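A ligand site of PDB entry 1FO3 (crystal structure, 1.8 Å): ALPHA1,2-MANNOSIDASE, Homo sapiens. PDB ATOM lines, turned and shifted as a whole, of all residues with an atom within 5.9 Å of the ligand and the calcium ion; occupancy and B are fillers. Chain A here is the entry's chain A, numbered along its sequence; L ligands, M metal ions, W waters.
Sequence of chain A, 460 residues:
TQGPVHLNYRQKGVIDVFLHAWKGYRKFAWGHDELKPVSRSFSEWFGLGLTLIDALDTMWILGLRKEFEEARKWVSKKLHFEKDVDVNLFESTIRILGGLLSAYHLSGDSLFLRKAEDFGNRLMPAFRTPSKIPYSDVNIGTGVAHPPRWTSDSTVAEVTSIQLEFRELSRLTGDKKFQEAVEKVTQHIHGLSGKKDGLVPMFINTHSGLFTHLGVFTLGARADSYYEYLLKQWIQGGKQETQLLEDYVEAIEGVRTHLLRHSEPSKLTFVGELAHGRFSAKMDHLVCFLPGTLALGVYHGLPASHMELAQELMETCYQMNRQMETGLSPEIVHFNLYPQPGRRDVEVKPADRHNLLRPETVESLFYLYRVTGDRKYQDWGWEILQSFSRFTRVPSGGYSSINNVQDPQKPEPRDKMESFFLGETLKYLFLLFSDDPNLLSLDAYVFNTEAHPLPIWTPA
OE1 of Glu 424 lies close to O2 of the ligand (2.7 Å). The side-chain carboxylate (OD2) of Asp 224 is in hydrogen-bond range of a nitrogen (N1) of the ligand, 3.1 Å away. An oxygen (O5) of the ligand lies within hydrogen-bond range of the guanidinium group (NH1) of Arg 358 (2.8 Å). An oxygen (O6) of the ligand sits at hydrogen-bond distance from the side-chain carboxylate of Glu 360. The side-chain carboxylate (OE1) of Glu 450 sits at hydrogen-bond distance from an oxygen (O1) of the ligand, 2.7 Å away.
The side-chain carboxylate (OE2) of Glu 228 lies close to the side-chain hydroxyl (OG1) of Thr 449 (2.7 Å). The side-chain carboxylate (OE1) of Glu 91 is in salt-bridge range of the guanidinium group (NH2) of Arg 95 (3.4 Å). N of Glu 450 sits close to ND2 of Asn 448 (2.8 Å). OE2 of Glu 450 is in salt-bridge range of NE of Arg 95 (3.5 Å). The backbone carbonyl oxygen (O) of Ile 94 sits close to the side-chain amide oxygen (OD1) of Asn 448 (3.0 Å). The side-chain carboxylate (OE2) of Glu 360 is in hydrogen-bond range of a ring nitrogen (ND1) of His 285 (3.0 Å).
CD1 of Ile 94 touches O1 of the ligand (3.8 Å). Arg 95 touches the ligand (NH2 to O1, 3.6 Å). CD1 of Leu 286 touches O4 of the ligand (3.0 Å). CD of Pro 359 touches O6 of the ligand (3.6 Å). Phe 420 touches the ligand. Hydrophobic or aromatic side chains that line the ligand: Ile 94, Leu 286, Pro 359 and Phe 420. 11 residues have an atom within 4 Å of the ligand: Ile 94, Arg 95, Asp 224, Leu 286, Arg 358, Pro 359, Glu 360, Phe 420, Glu 424, Thr 449 and Glu 450.
The nearest printed residue that does not touch the calcium ion is Glu 228 (4.2 Å).
Water W6 binds the calcium ion (2.4 Å). The calcium ion is bound by water W3 (2.4 Å). Water W11 binds the calcium ion. The calcium ion is bound by OG1 of Thr 449 (2.5 Å). An oxygen (O2) of the ligand is bound to the calcium ion, 2.5 Å away. O of Thr 449 is bound to the calcium ion (2.5 Å). The calcium ion is bound by water W10 (2.5 Å). The calcium ion is bound by an oxygen (O3) of the ligand (2.5 Å).
Water W10 bridges OE1 of Glu 228 (2.7 Å) and OE1 of Glu 363 (2.7 Å). Water W6 bridges the side-chain carboxylate of Glu 424 (2.6 Å) and the side-chain carboxylate of Glu 363 (2.7 Å). Water W1 lies within hydrogen-bond range of an oxygen (O1) of the ligand (2.7 Å), the side-chain carboxylate of Glu 91 (2.8 Å) and the guanidinium group of Arg 95 (3.5 Å). Water W5 lies within hydrogen-bond range of the guanidinium group of Arg 358 and an oxygen (O5) of the ligand. Water W4 lies within hydrogen-bond range of OD1 of Asp 224 (2.8 Å), N of Arg 222 (2.8 Å) and O4 of the ligand (3.1 Å). Water W8 bridges the side-chain carboxylate of Glu 91 (3.1 Å) and an oxygen (O5) of the ligand (3.3 Å).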
ATOM      1  N   PHE A  90     -33.920  16.552  13.289  1.00  0.00           N
ATOM      2  CA  PHE A  90     -32.560  16.835  13.752  1.00  0.00           C
ATOM      3  C   PHE A  90     -31.885  18.005  13.051  1.00  0.00           C
ATOM      4  O   PHE A  90     -31.445  18.948  13.717  1.00  0.00           O
ATOM      5  CB  PHE A  90     -31.705  15.555  13.625  1.00  0.00           C
ATOM      6  CG  PHE A  90     -30.216  15.810  13.625  1.00  0.00           C
ATOM      7  CD1 PHE A  90     -29.502  15.762  12.432  1.00  0.00           C
ATOM      8  CD2 PHE A  90     -29.534  16.060  14.807  1.00  0.00           C
ATOM      9  CE1 PHE A  90     -28.115  15.963  12.420  1.00  0.00           C
ATOM     10  CE2 PHE A  90     -28.148  16.267  14.802  1.00  0.00           C
ATOM     11  CZ  PHE A  90     -27.444  16.217  13.609  1.00  0.00           C
ATOM     12  N   GLU A  91     -31.822  17.960  11.724  1.00  0.00           N
ATOM     13  CA  GLU A  91     -31.178  19.024  10.959  1.00  0.00           C
ATOM     14  C   GLU A  91     -31.808  20.404  11.194  1.00  0.00           C
ATOM     15  O   GLU A  91     -31.093  21.408  11.276  1.00  0.00           O
ATOM     16  CB  GLU A  91     -31.214  18.701   9.461  1.00  0.00           C
ATOM     17  CG  GLU A  91     -30.526  17.392   9.056  1.00  0.00           C
ATOM     18  CD  GLU A  91     -29.006  17.428   9.212  1.00  0.00           C
ATOM     19  OE1 GLU A  91     -28.443  18.532   9.361  1.00  0.00           O
ATOM     20  OE2 GLU A  91     -28.375  16.355   9.175  1.00  0.00           O
ATOM     21  N   ILE A  94     -30.966  21.547  15.124  1.00  0.00           N
ATOM     22  CA  ILE A  94     -29.629  22.056  15.390  1.00  0.00           C
ATOM     23  C   ILE A  94     -29.311  23.341  14.627  1.00  0.00           C
ATOM     24  O   ILE A  94     -28.531  24.157  15.111  1.00  0.00           O
ATOM     25  CB  ILE A  94     -28.531  21.001  15.081  1.00  0.00           C
ATOM     26  CG1 ILE A  94     -28.481  20.702  13.577  1.00  0.00           C
ATOM     27  CG2 ILE A  94     -28.802  19.741  15.882  1.00  0.00           C
ATOM     28  CD1 ILE A  94     -27.341  19.746  13.187  1.00  0.00           C
ATOM     29  N   ARG A  95     -29.903  23.521  13.452  1.00  0.00           N
ATOM     30  CA  ARG A  95     -29.641  24.724  12.679  1.00  0.00           C
ATOM     31  C   ARG A  95     -30.602  25.867  12.968  1.00  0.00           C
ATOM     32  O   ARG A  95     -30.188  26.950  13.375  1.00  0.00           O
ATOM     33  CB  ARG A  95     -29.723  24.429  11.178  1.00  0.00           C
ATOM     34  CG  ARG A  95     -28.637  23.545  10.614  1.00  0.00           C
ATOM     35  CD  ARG A  95     -28.804  23.535   9.090  1.00  0.00           C
ATOM     36  NE  ARG A  95     -27.760  22.814   8.384  1.00  0.00           N
ATOM     37  CZ  ARG A  95     -27.483  21.522   8.547  1.00  0.00           C
ATOM     38  NH1 ARG A  95     -28.188  20.824   9.419  1.00  0.00           N
ATOM     39  NH2 ARG A  95     -26.556  20.936   7.813  1.00  0.00           N
ATOM     40  N   GLY A 220     -18.694   8.382  13.731  1.00  0.00           N
ATOM     41  CA  GLY A 220     -18.842   9.280  12.598  1.00  0.00           C
ATOM     42  C   GLY A 220     -20.299   9.560  12.291  1.00  0.00           C
ATOM     43  O   GLY A 220     -21.127   9.668  13.209  1.00  0.00           O
ATOM     44  N   ALA A 221     -20.623   9.675  11.015  1.00  0.00           N
ATOM     45  CA  ALA A 221     -21.989   9.958  10.606  1.00  0.00           C
ATOM     46  C   ALA A 221     -23.004   9.022  11.246  1.00  0.00           C
ATOM     47  O   ALA A 221     -22.773   7.808  11.357  1.00  0.00           O
ATOM     48  CB  ALA A 221     -22.093   9.880   9.078  1.00  0.00           C
ATOM     49  N   ARG A 222     -24.122   9.598  11.684  1.00  0.00           N
ATOM     50  CA  ARG A 222     -25.238   8.871  12.305  1.00  0.00           C
ATOM     51  C   ARG A 222     -25.088   8.598  13.799  1.00  0.00           C
ATOM     52  O   ARG A 222     -26.032   8.148  14.438  1.00  0.00           O
ATOM     53  CB  ARG A 222     -25.492   7.541  11.590  1.00  0.00           C
ATOM     54  CG  ARG A 222     -25.525   7.628  10.075  1.00  0.00           C
ATOM     55  CD  ARG A 222     -26.923   7.443   9.533  1.00  0.00           C
ATOM     56  NE  ARG A 222     -26.883   6.928   8.165  1.00  0.00           N
ATOM     57  CZ  ARG A 222     -27.959   6.765   7.389  1.00  0.00           C
ATOM     58  NH1 ARG A 222     -29.161   7.083   7.845  1.00  0.00           N
ATOM     59  NH2 ARG A 222     -27.824   6.285   6.159  1.00  0.00           N
ATOM     60  N   ASP A 224     -22.042  10.380  15.837  1.00  0.00           N
ATOM     61  CA  ASP A 224     -21.202  11.409  16.434  1.00  0.00           C
ATOM     62  C   ASP A 224     -21.781  12.244  17.586  1.00  0.00           C
ATOM     63  O   ASP A 224     -21.349  12.096  18.727  1.00  0.00           O
ATOM     64  CB  ASP A 224     -20.624  12.344  15.354  1.00  0.00           C
ATOM     65  CG  ASP A 224     -21.692  13.047  14.524  1.00  0.00           C
ATOM     66  OD1 ASP A 224     -22.899  12.810  14.726  1.00  0.00           O
ATOM     67  OD2 ASP A 224     -21.302  13.846  13.644  1.00  0.00           O
ATOM     68  N   SER A 225     -22.758  13.100  17.295  1.00  0.00           N
ATOM     69  CA  SER A 225     -23.293  13.973  18.338  1.00  0.00           C
ATOM     70  C   SER A 225     -24.005  13.310  19.521  1.00  0.00           C
ATOM     71  O   SER A 225     -24.296  13.974  20.516  1.00  0.00           O
ATOM     72  CB  SER A 225     -24.163  15.077  17.713  1.00  0.00           C
ATOM     73  OG  SER A 225     -25.140  14.553  16.845  1.00  0.00           O
ATOM     74  N   GLU A 228     -21.454  13.511  22.166  1.00  0.00           N
ATOM     75  CA  GLU A 228     -21.257  14.933  22.401  1.00  0.00           C
ATOM     76  C   GLU A 228     -22.336  15.507  23.324  1.00  0.00           C
ATOM     77  O   GLU A 228     -22.029  16.234  24.270  1.00  0.00           O
ATOM     78  CB  GLU A 228     -21.281  15.666  21.059  1.00  0.00           C
ATOM     79  CG  GLU A 228     -21.101  17.180  21.122  1.00  0.00           C
ATOM     80  CD  GLU A 228     -21.428  17.846  19.798  1.00  0.00           C
ATOM     81  OE1 GLU A 228     -21.360  19.092  19.706  1.00  0.00           O
ATOM     82  OE2 GLU A 228     -21.754  17.109  18.844  1.00  0.00           O
ATOM     83  N   HIS A 285     -14.063  12.621   8.947  1.00  0.00           N
ATOM     84  CA  HIS A 285     -13.559  13.869   9.495  1.00  0.00           C
ATOM     85  C   HIS A 285     -14.509  14.242  10.637  1.00  0.00           C
ATOM     86  O   HIS A 285     -14.119  14.911  11.588  1.00  0.00           O
ATOM     87  CB  HIS A 285     -13.551  14.963   8.428  1.00  0.00           C
ATOM     88  CG  HIS A 285     -13.083  16.297   8.932  1.00  0.00           C
ATOM     89  ND1 HIS A 285     -13.958  17.302   9.286  1.00  0.00           N
ATOM     90  CD2 HIS A 285     -11.840  16.769   9.173  1.00  0.00           C
ATOM     91  CE1 HIS A 285     -13.272  18.345   9.724  1.00  0.00           C
ATOM     92  NE2 HIS A 285     -11.983  18.047   9.669  1.00  0.00           N
ATOM     93  N   LEU A 286     -15.757  13.794  10.527  1.00  0.00           N
ATOM     94  CA  LEU A 286     -16.767  14.063  11.550  1.00  0.00           C
ATOM     95  C   LEU A 286     -16.267  13.663  12.926  1.00  0.00           C
ATOM     96  O   LEU A 286     -16.595  14.304  13.933  1.00  0.00           O
ATOM     97  CB  LEU A 286     -18.069  13.312  11.244  1.00  0.00           C
ATOM     98  CG  LEU A 286     -18.844  13.708   9.994  1.00  0.00           C
ATOM     99  CD1 LEU A 286     -20.094  12.844   9.893  1.00  0.00           C
ATOM    100  CD2 LEU A 286     -19.230  15.200  10.067  1.00  0.00           C
ATOM    101  N   PHE A 289     -14.583  15.787  16.019  1.00  0.00           N
ATOM    102  CA  PHE A 289     -15.306  16.581  17.005  1.00  0.00           C
ATOM    103  C   PHE A 289     -14.850  16.093  18.378  1.00  0.00           C
ATOM    104  O   PHE A 289     -14.841  16.831  19.362  1.00  0.00           O
ATOM    105  CB  PHE A 289     -16.820  16.353  16.881  1.00  0.00           C
ATOM    106  CG  PHE A 289     -17.323  15.136  17.629  1.00  0.00           C
ATOM    107  CD1 PHE A 289     -17.657  15.213  18.981  1.00  0.00           C
ATOM    108  CD2 PHE A 289     -17.402  13.901  16.995  1.00  0.00           C
ATOM    109  CE1 PHE A 289     -18.063  14.072  19.687  1.00  0.00           C
ATOM    110  CE2 PHE A 289     -17.797  12.756  17.692  1.00  0.00           C
ATOM    111  CZ  PHE A 289     -18.132  12.840  19.039  1.00  0.00           C
ATOM    112  N   ARG A 358     -16.132  21.545   6.278  1.00  0.00           N
ATOM    113  CA  ARG A 358     -16.549  21.101   7.606  1.00  0.00           C
ATOM    114  C   ARG A 358     -15.737  21.738   8.743  1.00  0.00           C
ATOM    115  O   ARG A 358     -14.546  22.004   8.616  1.00  0.00           O
ATOM    116  CB  ARG A 358     -16.514  19.577   7.694  1.00  0.00           C
ATOM    117  CG  ARG A 358     -17.573  18.893   6.820  1.00  0.00           C
ATOM    118  CD  ARG A 358     -17.520  17.385   7.024  1.00  0.00           C
ATOM    119  NE  ARG A 358     -18.339  16.618   6.083  1.00  0.00           N
ATOM    120  CZ  ARG A 358     -19.665  16.527   6.123  1.00  0.00           C
ATOM    121  NH1 ARG A 358     -20.357  17.151   7.064  1.00  0.00           N
ATOM    122  NH2 ARG A 358     -20.292  15.766   5.243  1.00  0.00           N
ATOM    123  N   PRO A 359     -16.392  21.953   9.907  1.00  0.00           N
ATOM    124  CA  PRO A 359     -15.830  22.569  11.111  1.00  0.00           C
ATOM    125  C   PRO A 359     -15.087  21.751  12.169  1.00  0.00           C
ATOM    126  O   PRO A 359     -14.385  22.331  12.994  1.00  0.00           O
ATOM    127  CB  PRO A 359     -17.063  23.207  11.738  1.00  0.00           C
ATOM    128  CG  PRO A 359     -18.085  22.111  11.530  1.00  0.00           C
ATOM    129  CD  PRO A 359     -17.840  21.697  10.077  1.00  0.00           C
ATOM    130  N   GLU A 360     -15.235  20.442  12.133  1.00  0.00           N
ATOM    131  CA  GLU A 360     -14.653  19.616  13.187  1.00  0.00           C
ATOM    132  C   GLU A 360     -13.205  19.813  13.651  1.00  0.00           C
ATOM    133  O   GLU A 360     -12.939  19.734  14.854  1.00  0.00           O
ATOM    134  CB  GLU A 360     -14.910  18.140  12.895  1.00  0.00           C
ATOM    135  CG  GLU A 360     -16.400  17.783  12.896  1.00  0.00           C
ATOM    136  CD  GLU A 360     -17.082  18.124  11.587  1.00  0.00           C
ATOM    137  OE1 GLU A 360     -18.337  18.136  11.560  1.00  0.00           O
ATOM    138  OE2 GLU A 360     -16.394  18.372  10.584  1.00  0.00           O
ATOM    139  N   GLU A 363     -13.064  23.327  15.231  1.00  0.00           N
ATOM    140  CA  GLU A 363     -13.922  23.276  16.414  1.00  0.00           C
ATOM    141  C   GLU A 363     -13.097  22.720  17.577  1.00  0.00           C
ATOM    142  O   GLU A 363     -13.054  23.282  18.671  1.00  0.00           O
ATOM    143  CB  GLU A 363     -15.130  22.354  16.161  1.00  0.00           C
ATOM    144  CG  GLU A 363     -15.901  21.945  17.423  1.00  0.00           C
ATOM    145  CD  GLU A 363     -17.050  20.981  17.135  1.00  0.00           C
ATOM    146  OE1 GLU A 363     -17.751  20.586  18.083  1.00  0.00           O
ATOM    147  OE2 GLU A 363     -17.246  20.634  15.958  1.00  0.00           O
ATOM    148  N   PHE A 420     -23.080  25.303   7.454  1.00  0.00           N
ATOM    149  CA  PHE A 420     -22.159  25.207   8.576  1.00  0.00           C
ATOM    150  C   PHE A 420     -20.793  25.844   8.373  1.00  0.00           C
ATOM    151  O   PHE A 420     -20.008  25.929   9.316  1.00  0.00           O
ATOM    152  CB  PHE A 420     -22.015  23.752   9.056  1.00  0.00           C
ATOM    153  CG  PHE A 420     -21.680  22.753   7.966  1.00  0.00           C
ATOM    154  CD1 PHE A 420     -20.435  22.747   7.358  1.00  0.00           C
ATOM    155  CD2 PHE A 420     -22.614  21.783   7.600  1.00  0.00           C
ATOM    156  CE1 PHE A 420     -20.107  21.787   6.402  1.00  0.00           C
ATOM    157  CE2 PHE A 420     -22.304  20.811   6.650  1.00  0.00           C
ATOM    158  CZ  PHE A 420     -21.041  20.815   6.050  1.00  0.00           C
ATOM    159  N   GLU A 424     -20.555  27.439  11.564  1.00  0.00           N
ATOM    160  CA  GLU A 424     -19.574  26.765  12.436  1.00  0.00           C
ATOM    161  C   GLU A 424     -18.101  27.050  12.198  1.00  0.00           C
ATOM    162  O   GLU A 424     -17.410  27.578  13.059  1.00  0.00           O
ATOM    163  CB  GLU A 424     -19.755  25.254  12.345  1.00  0.00           C
ATOM    164  CG  GLU A 424     -21.153  24.735  12.643  1.00  0.00           C
ATOM    165  CD  GLU A 424     -21.102  23.282  13.083  1.00  0.00           C
ATOM    166  OE1 GLU A 424     -21.797  22.451  12.459  1.00  0.00           O
ATOM    167  OE2 GLU A 424     -20.346  22.991  14.025  1.00  0.00           O
ATOM    168  N   ASN A 448     -24.192  24.172  20.829  1.00  0.00           N
ATOM    169  CA  ASN A 448     -24.948  23.015  20.378  1.00  0.00           C
ATOM    170  C   ASN A 448     -24.078  22.417  19.279  1.00  0.00           C
ATOM    171  O   ASN A 448     -22.983  22.925  19.008  1.00  0.00           O
ATOM    172  CB  ASN A 448     -26.391  23.383  19.932  1.00  0.00           C
ATOM    173  CG  ASN A 448     -26.511  23.765  18.473  1.00  0.00           C
ATOM    174  OD1 ASN A 448     -27.577  23.543  17.868  1.00  0.00           O
ATOM    175  ND2 ASN A 448     -25.479  24.338  17.905  1.00  0.00           N
ATOM    176  N   THR A 449     -24.533  21.337  18.638  1.00  0.00           N
ATOM    177  CA  THR A 449     -23.676  20.699  17.655  1.00  0.00           C
ATOM    178  C   THR A 449     -23.505  21.426  16.307  1.00  0.00           C
ATOM    179  O   THR A 449     -22.755  20.971  15.437  1.00  0.00           O
ATOM    180  CB  THR A 449     -24.094  19.209  17.451  1.00  0.00           C
ATOM    181  OG1 THR A 449     -23.010  18.497  16.846  1.00  0.00           O
ATOM    182  CG2 THR A 449     -25.329  19.076  16.605  1.00  0.00           C
ATOM    183  N   GLU A 450     -24.170  22.569  16.162  1.00  0.00           N
ATOM    184  CA  GLU A 450     -24.046  23.378  14.947  1.00  0.00           C
ATOM    185  C   GLU A 450     -23.495  24.755  15.368  1.00  0.00           C
ATOM    186  O   GLU A 450     -23.823  25.789  14.786  1.00  0.00           O
ATOM    187  CB  GLU A 450     -25.406  23.524  14.227  1.00  0.00           C
ATOM    188  CG  GLU A 450     -25.350  24.211  12.855  1.00  0.00           C
ATOM    189  CD  GLU A 450     -25.186  23.258  11.667  1.00  0.00           C
ATOM    190  OE1 GLU A 450     -25.135  22.027  11.865  1.00  0.00           O
ATOM    191  OE2 GLU A 450     -25.123  23.749  10.518  1.00  0.00           O
HETATM  192  C1  LIG L   1     -23.172  19.963  10.852  1.00  0.00           C
HETATM  193  O1  LIG L   1     -24.562  19.731  10.560  1.00  0.00           O
HETATM  194  C2  LIG L   1     -22.972  19.586  12.381  1.00  0.00           C
HETATM  195  O2  LIG L   1     -21.653  19.820  12.875  1.00  0.00           O
HETATM  196  C3  LIG L   1     -23.311  18.051  12.611  1.00  0.00           C
HETATM  197  O3  LIG L   1     -23.066  17.707  13.973  1.00  0.00           O
HETATM  198  C4  LIG L   1     -22.414  17.201  11.642  1.00  0.00           C
HETATM  199  N1  LIG L   1     -22.774  15.774  11.752  1.00  0.00           N
HETATM  200  C5  LIG L   1     -22.796  15.375  10.450  1.00  0.00           C
HETATM  201  O4  LIG L   1     -22.808  14.210  10.088  1.00  0.00           O
HETATM  202  C6  LIG L   1     -22.804  16.552   9.545  1.00  0.00           C
HETATM  203  O5  LIG L   1     -22.828  16.535   8.323  1.00  0.00           O
HETATM  204  N2  LIG L   1     -22.824  17.609  10.336  1.00  0.00           N
HETATM  205  C7  LIG L   1     -22.406  19.002   9.871  1.00  0.00           C
HETATM  206  C8  LIG L   1     -20.863  19.239   9.867  1.00  0.00           C
HETATM  207  O6  LIG L   1     -19.620  18.648   9.446  1.00  0.00           O
HETATM  208 CA    CA M   1     -21.239  18.999  15.181  1.00  0.00          CA
HETATM  209  O   HOH W   1     -25.758  17.801   9.052  1.00  0.00           O
HETATM  210  O   HOH W   2     -24.936  17.687   6.327  1.00  0.00           O
HETATM  211  O   HOH W   3     -19.757  17.708  13.747  1.00  0.00           O
HETATM  212  O   HOH W   4     -24.015  12.340  12.227  1.00  0.00           O
HETATM  213  O   HOH W   5     -23.123  15.447   5.487  1.00  0.00           O
HETATM  214  O   HOH W   6     -19.515  20.598  14.564  1.00  0.00           O
HETATM  215  O   HOH W   7     -24.240  15.367  14.407  1.00  0.00           O
HETATM  216  O   HOH W   8     -25.754  15.117   8.129  1.00  0.00           O
HETATM  217  O   HOH W   9     -23.149  13.529   7.393  1.00  0.00           O
HETATM  218  O   HOH W  10     -20.305  19.897  17.335  1.00  0.00           O
HETATM  219  O   HOH W  11     -20.667  16.837  16.213  1.00  0.00           O
